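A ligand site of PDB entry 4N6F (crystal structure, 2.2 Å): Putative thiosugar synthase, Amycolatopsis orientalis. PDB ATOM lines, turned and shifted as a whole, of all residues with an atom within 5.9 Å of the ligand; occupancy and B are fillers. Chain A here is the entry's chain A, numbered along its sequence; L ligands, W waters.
The side-chain amino group (NZ) of Lys 110 is covalently linked to a carbon (C1) of the ligand (1.5 Å). An oxygen (O3) of the ligand is in hydrogen-bond range of the side-chain carboxylate (OE1) of Glu 194, 2.5 Å away. The backbone NH (N) of Thr 218 sits at hydrogen-bond distance from an oxygen (O6) of the ligand (3.2 Å). O6 of the ligand is in hydrogen-bond range of OG1 of Thr 218, 2.6 Å away. The side-chain carboxylate (OE1) of Glu 31 sits close to an oxygen (O1) of the ligand (2.7 Å). O3 of the ligand lies within hydrogen-bond range of NH2 of Arg 114, at 2.7 Å. O8 of the ligand is in hydrogen-bond range of N of Ala 169 (2.8 Å). O8 of the ligand is in hydrogen-bond range of N of Gly 196 (2.9 Å). O7 of the ligand is in hydrogen-bond range of N of Asn 217. ND2 of Asn 217 lies within hydrogen-bond range of O4 of the ligand, 3.1 Å away.
CA of Gly 29 touches O1 of the ligand, 3.7 Å away. CB of Ser 85 touches C1 of the ligand, 3.96 Å away. Asp 112 touches the ligand (OD2 to C1, 3.1 Å). Phe 142 touches the ligand (CE2 to O3, 3.7 Å). NH1 of Arg 162 touches C1 of the ligand, at 3.3 Å. Val 168 touches the ligand. CA of Gly 195 touches O5 of the ligand, at 3.5 Å. Within 4 Å of the ligand: Gly 29, Glu 31, Ser 85, Lys 110, Asp 112, Arg 114, Phe 142, Arg 162, Val 168, Ala 169, Glu 194, Gly 195, Gly 196, Asn 217 and Thr 218. The nearest printed residue that does not touch the ligand is Val 216 (4.02 Å).
Water W3 lies within hydrogen-bond range of an oxygen (O7) of the ligand (2.6 Å), the backbone NH of Gly 195 (2.8 Å), the backbone carbonyl oxygen of Leu 215 (2.8 Å) and the backbone NH of Ile 197 (3.5 Å). Water W4 lies within hydrogen-bond range of an oxygen (O8) of the ligand, the backbone carbonyl oxygen (O) of Ile 197 and the backbone NH (N) of Gly 171.
The guanidinium group (NE) of Arg 162 is in salt-bridge range of the side-chain carboxylate (OE2) of Glu 194 (2.6 Å). The side-chain carboxylate (OE2) of Glu 31 is in hydrogen-bond range of the side-chain hydroxyl (OG) of Ser 85 (2.9 Å). The side-chain carboxylate of Glu 31 is in hydrogen-bond range of the side-chain hydroxyl of Thr 83. OD1 of Asp 112 lies within salt-bridge range of NH2 of Arg 114. The backbone NH (N) of Gly 196 sits close to the backbone carbonyl oxygen (O) of Pro 167, 3.4 Å away. O of Gly 196 sits close to N of Gly 171, 3.5 Å away. The guanidinium group of Arg 162 lies within salt-bridge range of the side-chain carboxylate of Asp 112 (2.8 Å). OD1 of Asn 217 sits close to O of Gly 29 (3.4 Å).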
ATOM      1  N   GLY A  29      18.153 -20.606  19.703  1.00  0.00           N
ATOM      2  CA  GLY A  29      16.858 -20.992  20.243  1.00  0.00           C
ATOM      3  C   GLY A  29      15.820 -20.770  19.179  1.00  0.00           C
ATOM      4  O   GLY A  29      15.158 -19.733  19.156  1.00  0.00           O
ATOM      5  N   ILE A  30      15.686 -21.759  18.298  1.00  0.00           N
ATOM      6  CA  ILE A  30      14.836 -21.659  17.111  1.00  0.00           C
ATOM      7  C   ILE A  30      13.406 -22.145  17.332  1.00  0.00           C
ATOM      8  O   ILE A  30      12.577 -22.002  16.434  1.00  0.00           O
ATOM      9  CB  ILE A  30      15.385 -22.512  15.929  1.00  0.00           C
ATOM     10  CG1 ILE A  30      15.507 -23.983  16.334  1.00  0.00           C
ATOM     11  CG2 ILE A  30      16.732 -21.965  15.447  1.00  0.00           C
ATOM     12  CD1 ILE A  30      15.589 -24.931  15.169  1.00  0.00           C
ATOM     13  N   GLU A  31      13.128 -22.743  18.490  1.00  0.00           N
ATOM     14  CA  GLU A  31      11.913 -23.565  18.636  1.00  0.00           C
ATOM     15  C   GLU A  31      10.599 -22.834  18.288  1.00  0.00           C
ATOM     16  O   GLU A  31       9.631 -23.489  17.912  1.00  0.00           O
ATOM     17  CB  GLU A  31      11.834 -24.277  20.010  1.00  0.00           C
ATOM     18  CG  GLU A  31      11.871 -23.398  21.265  1.00  0.00           C
ATOM     19  CD  GLU A  31      13.212 -23.459  21.996  1.00  0.00           C
ATOM     20  OE1 GLU A  31      14.201 -22.968  21.421  1.00  0.00           O
ATOM     21  OE2 GLU A  31      13.279 -23.989  23.134  1.00  0.00           O
ATOM     22  N   ILE A  52      17.529 -27.718  18.082  1.00  0.00           N
ATOM     23  CA  ILE A  52      16.554 -27.769  19.140  1.00  0.00           C
ATOM     24  C   ILE A  52      15.215 -28.024  18.509  1.00  0.00           C
ATOM     25  O   ILE A  52      14.727 -27.226  17.787  1.00  0.00           O
ATOM     26  CB  ILE A  52      16.545 -26.496  19.968  1.00  0.00           C
ATOM     27  CG1 ILE A  52      17.832 -26.346  20.759  1.00  0.00           C
ATOM     28  CG2 ILE A  52      15.389 -26.502  20.924  1.00  0.00           C
ATOM     29  CD1 ILE A  52      18.148 -24.945  21.113  1.00  0.00           C
ATOM     30  N   THR A  83      12.940 -29.877  23.940  1.00  0.00           N
ATOM     31  CA  THR A  83      12.713 -28.709  24.756  1.00  0.00           C
ATOM     32  C   THR A  83      11.375 -28.802  25.515  1.00  0.00           C
ATOM     33  O   THR A  83      10.443 -29.469  25.046  1.00  0.00           O
ATOM     34  CB  THR A  83      12.757 -27.419  23.926  1.00  0.00           C
ATOM     35  OG1 THR A  83      12.436 -26.308  24.754  1.00  0.00           O
ATOM     36  CG2 THR A  83      11.766 -27.479  22.763  1.00  0.00           C
ATOM     37  N   SER A  85      10.220 -25.655  26.666  1.00  0.00           N
ATOM     38  CA  SER A  85       9.961 -24.202  26.761  1.00  0.00           C
ATOM     39  C   SER A  85       8.524 -23.790  26.398  1.00  0.00           C
ATOM     40  O   SER A  85       8.099 -22.681  26.741  1.00  0.00           O
ATOM     41  CB  SER A  85      10.964 -23.402  25.929  1.00  0.00           C
ATOM     42  OG  SER A  85      10.759 -23.607  24.547  1.00  0.00           O
ATOM     43  N   LYS A 110      16.496 -29.644  26.689  1.00  0.00           N
ATOM     44  CA  LYS A 110      16.533 -28.245  27.073  1.00  0.00           C
ATOM     45  C   LYS A 110      15.379 -28.067  28.024  1.00  0.00           C
ATOM     46  O   LYS A 110      14.225 -28.052  27.614  1.00  0.00           O
ATOM     47  CB  LYS A 110      16.475 -27.371  25.819  1.00  0.00           C
ATOM     48  CG  LYS A 110      16.334 -25.879  26.065  1.00  0.00           C
ATOM     49  CD  LYS A 110      16.327 -25.125  24.742  1.00  0.00           C
ATOM     50  CE  LYS A 110      16.214 -23.616  24.908  1.00  0.00           C
ATOM     51  NZ  LYS A 110      14.802 -23.251  25.161  1.00  0.00           N
ATOM     52  N   ASP A 112      13.107 -26.164  30.589  1.00  0.00           N
ATOM     53  CA  ASP A 112      12.627 -24.844  30.964  1.00  0.00           C
ATOM     54  C   ASP A 112      11.358 -24.988  31.800  1.00  0.00           C
ATOM     55  O   ASP A 112      10.398 -25.652  31.388  1.00  0.00           O
ATOM     56  CB  ASP A 112      12.334 -24.033  29.697  1.00  0.00           C
ATOM     57  CG  ASP A 112      13.593 -23.521  29.014  1.00  0.00           C
ATOM     58  OD1 ASP A 112      14.297 -22.714  29.621  1.00  0.00           O
ATOM     59  OD2 ASP A 112      13.863 -23.922  27.863  1.00  0.00           O
ATOM     60  N   ARG A 114       9.227 -22.110  33.845  1.00  0.00           N
ATOM     61  CA  ARG A 114       9.182 -20.661  34.068  1.00  0.00           C
ATOM     62  C   ARG A 114       7.933 -20.186  34.801  1.00  0.00           C
ATOM     63  O   ARG A 114       6.866 -20.784  34.681  1.00  0.00           O
ATOM     64  CB  ARG A 114       9.284 -19.928  32.742  1.00  0.00           C
ATOM     65  CG  ARG A 114      10.460 -20.415  31.926  1.00  0.00           C
ATOM     66  CD  ARG A 114      10.725 -19.547  30.719  1.00  0.00           C
ATOM     67  NE  ARG A 114      11.928 -20.003  30.043  1.00  0.00           N
ATOM     68  CZ  ARG A 114      12.434 -19.453  28.943  1.00  0.00           C
ATOM     69  NH1 ARG A 114      11.836 -18.417  28.359  1.00  0.00           N
ATOM     70  NH2 ARG A 114      13.548 -19.963  28.420  1.00  0.00           N
ATOM     71  N   ASN A 118       7.960 -15.049  32.646  1.00  0.00           N
ATOM     72  CA  ASN A 118       8.938 -15.583  31.682  1.00  0.00           C
ATOM     73  C   ASN A 118      10.363 -15.662  32.249  1.00  0.00           C
ATOM     74  O   ASN A 118      11.354 -15.524  31.521  1.00  0.00           O
ATOM     75  CB  ASN A 118       8.905 -14.783  30.387  1.00  0.00           C
ATOM     76  CG  ASN A 118       9.377 -15.582  29.184  1.00  0.00           C
ATOM     77  OD1 ASN A 118       9.384 -16.808  29.212  1.00  0.00           O
ATOM     78  ND2 ASN A 118       9.775 -14.882  28.126  1.00  0.00           N
ATOM     79  N   PHE A 142      17.617 -24.190  32.758  1.00  0.00           N
ATOM     80  CA  PHE A 142      17.785 -22.742  32.712  1.00  0.00           C
ATOM     81  C   PHE A 142      17.461 -22.210  34.108  1.00  0.00           C
ATOM     82  O   PHE A 142      16.411 -22.548  34.674  1.00  0.00           O
ATOM     83  CB  PHE A 142      16.801 -22.168  31.679  1.00  0.00           C
ATOM     84  CG  PHE A 142      17.048 -20.736  31.291  1.00  0.00           C
ATOM     85  CD1 PHE A 142      18.294 -20.144  31.370  1.00  0.00           C
ATOM     86  CD2 PHE A 142      16.001 -19.986  30.779  1.00  0.00           C
ATOM     87  CE1 PHE A 142      18.484 -18.821  30.988  1.00  0.00           C
ATOM     88  CE2 PHE A 142      16.180 -18.663  30.383  1.00  0.00           C
ATOM     89  CZ  PHE A 142      17.426 -18.084  30.490  1.00  0.00           C
ATOM     90  N   ARG A 162      22.271 -23.638  31.847  1.00  0.00           N
ATOM     91  CA  ARG A 162      21.986 -22.377  31.169  1.00  0.00           C
ATOM     92  C   ARG A 162      21.656 -21.365  32.263  1.00  0.00           C
ATOM     93  O   ARG A 162      20.841 -21.645  33.152  1.00  0.00           O
ATOM     94  CB  ARG A 162      20.842 -22.550  30.170  1.00  0.00           C
ATOM     95  CG  ARG A 162      21.153 -23.541  29.041  1.00  0.00           C
ATOM     96  CD  ARG A 162      19.914 -24.301  28.570  1.00  0.00           C
ATOM     97  NE  ARG A 162      18.843 -23.389  28.210  1.00  0.00           N
ATOM     98  CZ  ARG A 162      17.547 -23.548  28.495  1.00  0.00           C
ATOM     99  NH1 ARG A 162      16.688 -22.601  28.120  1.00  0.00           N
ATOM    100  NH2 ARG A 162      17.102 -24.612  29.141  1.00  0.00           N
ATOM    101  N   PRO A 167      16.720 -10.230  31.212  1.00  0.00           N
ATOM    102  CA  PRO A 167      15.420 -10.756  30.836  1.00  0.00           C
ATOM    103  C   PRO A 167      15.301 -11.133  29.364  1.00  0.00           C
ATOM    104  O   PRO A 167      15.921 -10.505  28.506  1.00  0.00           O
ATOM    105  CB  PRO A 167      14.456  -9.617  31.202  1.00  0.00           C
ATOM    106  CG  PRO A 167      15.149  -8.879  32.292  1.00  0.00           C
ATOM    107  CD  PRO A 167      16.609  -8.932  31.908  1.00  0.00           C
ATOM    108  N   VAL A 168      14.502 -12.164  29.120  1.00  0.00           N
ATOM    109  CA  VAL A 168      14.286 -12.700  27.783  1.00  0.00           C
ATOM    110  C   VAL A 168      13.741 -11.621  26.857  1.00  0.00           C
ATOM    111  O   VAL A 168      12.818 -10.895  27.219  1.00  0.00           O
ATOM    112  CB  VAL A 168      13.322 -13.896  27.818  1.00  0.00           C
ATOM    113  CG1 VAL A 168      12.920 -14.337  26.414  1.00  0.00           C
ATOM    114  CG2 VAL A 168      13.986 -15.054  28.538  1.00  0.00           C
ATOM    115  N   ALA A 169      14.323 -11.540  25.662  1.00  0.00           N
ATOM    116  CA  ALA A 169      13.904 -10.608  24.601  1.00  0.00           C
ATOM    117  C   ALA A 169      14.252  -9.162  24.875  1.00  0.00           C
ATOM    118  O   ALA A 169      13.878  -8.281  24.112  1.00  0.00           O
ATOM    119  CB  ALA A 169      12.402 -10.736  24.291  1.00  0.00           C
ATOM    120  N   SER A 170      15.041  -8.915  25.920  1.00  0.00           N
ATOM    121  CA  SER A 170      15.288  -7.549  26.362  1.00  0.00           C
ATOM    122  C   SER A 170      16.496  -6.906  25.705  1.00  0.00           C
ATOM    123  O   SER A 170      16.630  -5.687  25.744  1.00  0.00           O
ATOM    124  CB  SER A 170      15.454  -7.522  27.878  1.00  0.00           C
ATOM    125  OG  SER A 170      16.727  -7.986  28.269  1.00  0.00           O
ATOM    126  N   GLY A 171      17.418  -7.708  25.161  1.00  0.00           N
ATOM    127  CA  GLY A 171      18.629  -7.177  24.535  1.00  0.00           C
ATOM    128  C   GLY A 171      19.561  -6.404  25.461  1.00  0.00           C
ATOM    129  O   GLY A 171      20.431  -5.661  24.996  1.00  0.00           O
ATOM    130  N   GLU A 194      22.566 -17.210  28.650  1.00  0.00           N
ATOM    131  CA  GLU A 194      21.324 -17.170  27.888  1.00  0.00           C
ATOM    132  C   GLU A 194      20.347 -16.151  28.470  1.00  0.00           C
ATOM    133  O   GLU A 194      20.286 -15.954  29.684  1.00  0.00           O
ATOM    134  CB  GLU A 194      20.697 -18.561  27.875  1.00  0.00           C
ATOM    135  CG  GLU A 194      19.344 -18.689  27.171  1.00  0.00           C
ATOM    136  CD  GLU A 194      18.853 -20.125  27.120  1.00  0.00           C
ATOM    137  OE1 GLU A 194      17.638 -20.335  26.867  1.00  0.00           O
ATOM    138  OE2 GLU A 194      19.669 -21.060  27.355  1.00  0.00           O
ATOM    139  N   GLY A 195      19.594 -15.496  27.590  1.00  0.00           N
ATOM    140  CA  GLY A 195      18.567 -14.557  27.985  1.00  0.00           C
ATOM    141  C   GLY A 195      19.034 -13.116  27.902  1.00  0.00           C
ATOM    142  O   GLY A 195      19.945 -12.702  28.612  1.00  0.00           O
ATOM    143  N   GLY A 196      18.398 -12.355  27.016  1.00  0.00           N
ATOM    144  CA  GLY A 196      18.673 -10.930  26.925  1.00  0.00           C
ATOM    145  C   GLY A 196      19.918 -10.570  26.140  1.00  0.00           C
ATOM    146  O   GLY A 196      20.318  -9.406  26.123  1.00  0.00           O
ATOM    147  N   ILE A 197      20.534 -11.553  25.483  1.00  0.00           N
ATOM    148  CA  ILE A 197      21.650 -11.286  24.606  1.00  0.00           C
ATOM    149  C   ILE A 197      21.129 -10.471  23.417  1.00  0.00           C
ATOM    150  O   ILE A 197      20.125 -10.812  22.786  1.00  0.00           O
ATOM    151  CB  ILE A 197      22.329 -12.567  24.083  1.00  0.00           C
ATOM    152  CG1 ILE A 197      22.887 -13.406  25.235  1.00  0.00           C
ATOM    153  CG2 ILE A 197      23.448 -12.211  23.111  1.00  0.00           C
ATOM    154  CD1 ILE A 197      23.960 -12.717  26.046  1.00  0.00           C
ATOM    155  N   LEU A 215      23.460 -18.984  24.249  1.00  0.00           N
ATOM    156  CA  LEU A 215      22.254 -19.287  23.495  1.00  0.00           C
ATOM    157  C   LEU A 215      21.611 -17.971  23.131  1.00  0.00           C
ATOM    158  O   LEU A 215      21.363 -17.134  23.993  1.00  0.00           O
ATOM    159  CB  LEU A 215      21.286 -20.155  24.292  1.00  0.00           C
ATOM    160  CG  LEU A 215      20.111 -20.696  23.466  1.00  0.00           C
ATOM    161  CD1 LEU A 215      19.670 -22.077  23.951  1.00  0.00           C
ATOM    162  CD2 LEU A 215      18.922 -19.745  23.441  1.00  0.00           C
ATOM    163  N   VAL A 216      21.376 -17.795  21.860  1.00  0.00           N
ATOM    164  CA  VAL A 216      20.770 -16.607  21.336  1.00  0.00           C
ATOM    165  C   VAL A 216      19.492 -16.934  20.585  1.00  0.00           C
ATOM    166  O   VAL A 216      19.365 -17.977  20.038  1.00  0.00           O
ATOM    167  CB  VAL A 216      21.721 -15.804  20.463  1.00  0.00           C
ATOM    168  CG1 VAL A 216      22.951 -15.459  21.243  1.00  0.00           C
ATOM    169  CG2 VAL A 216      22.095 -16.548  19.212  1.00  0.00           C
ATOM    170  N   ASN A 217      18.543 -16.031  20.660  1.00  0.00           N
ATOM    171  CA  ASN A 217      17.285 -16.088  19.957  1.00  0.00           C
ATOM    172  C   ASN A 217      16.800 -14.738  19.425  1.00  0.00           C
ATOM    173  O   ASN A 217      16.916 -14.461  18.274  1.00  0.00           O
ATOM    174  CB  ASN A 217      16.227 -16.705  20.864  1.00  0.00           C
ATOM    175  CG  ASN A 217      14.852 -16.745  20.228  1.00  0.00           C
ATOM    176  OD1 ASN A 217      14.693 -16.392  19.112  1.00  0.00           O
ATOM    177  ND2 ASN A 217      13.891 -17.176  20.957  1.00  0.00           N
ATOM    178  N   THR A 218      16.334 -13.865  20.300  1.00  0.00           N
ATOM    179  CA  THR A 218      15.779 -12.583  19.934  1.00  0.00           C
ATOM    180  C   THR A 218      16.752 -11.665  19.185  1.00  0.00           C
ATOM    181  O   THR A 218      16.362 -10.984  18.314  1.00  0.00           O
ATOM    182  CB  THR A 218      15.213 -11.849  21.156  1.00  0.00           C
ATOM    183  OG1 THR A 218      14.156 -12.591  21.712  1.00  0.00           O
ATOM    184  CG2 THR A 218      14.691 -10.521  20.781  1.00  0.00           C
ATOM    185  N   ALA A 219      18.017 -11.654  19.556  1.00  0.00           N
ATOM    186  CA  ALA A 219      19.028 -10.820  18.892  1.00  0.00           C
ATOM    187  C   ALA A 219      19.158 -11.059  17.380  1.00  0.00           C
ATOM    188  O   ALA A 219      19.489 -10.140  16.622  1.00  0.00           O
ATOM    189  CB  ALA A 219      20.387 -11.020  19.535  1.00  0.00           C
HETATM  190  C1  LIG L   1      14.600 -21.868  25.660  1.00  0.00           C
HETATM  191  C2  LIG L   1      14.544 -20.885  24.523  1.00  0.00           C
HETATM  192  C3  LIG L   1      14.167 -19.435  24.720  1.00  0.00           C
HETATM  193  C4  LIG L   1      15.358 -18.703  25.328  1.00  0.00           C
HETATM  194  C5  LIG L   1      15.217 -17.187  25.198  1.00  0.00           C
HETATM  195  C6  LIG L   1      16.570 -16.503  25.285  1.00  0.00           C
HETATM  196  O1  LIG L   1      14.878 -21.239  23.390  1.00  0.00           O
HETATM  197  O2  LIG L   1      13.001 -19.240  25.537  1.00  0.00           O
HETATM  198  O3  LIG L   1      15.466 -19.044  26.728  1.00  0.00           O
HETATM  199  O4  LIG L   1      14.615 -16.822  23.968  1.00  0.00           O
HETATM  200  O5  LIG L   1      16.356 -15.098  25.323  1.00  0.00           O
HETATM  201  P1  LIG L   1      16.534 -14.148  24.052  1.00  0.00           P
HETATM  202  O6  LIG L   1      15.309 -14.416  23.249  1.00  0.00           O
HETATM  203  O7  LIG L   1      17.810 -14.560  23.366  1.00  0.00           O
HETATM  204  O8  LIG L   1      16.656 -12.796  24.711  1.00  0.00           O
HETATM  205  O   HOH W   1      11.607 -16.467  23.853  1.00  0.00           O
HETATM  206  O   HOH W   2      19.195 -13.134  21.776  1.00  0.00           O
HETATM  207  O   HOH W   3      19.905 -14.924  24.896  1.00  0.00           O
HETATM  208  O   HOH W   4      17.479 -10.361  23.832  1.00  0.00           O
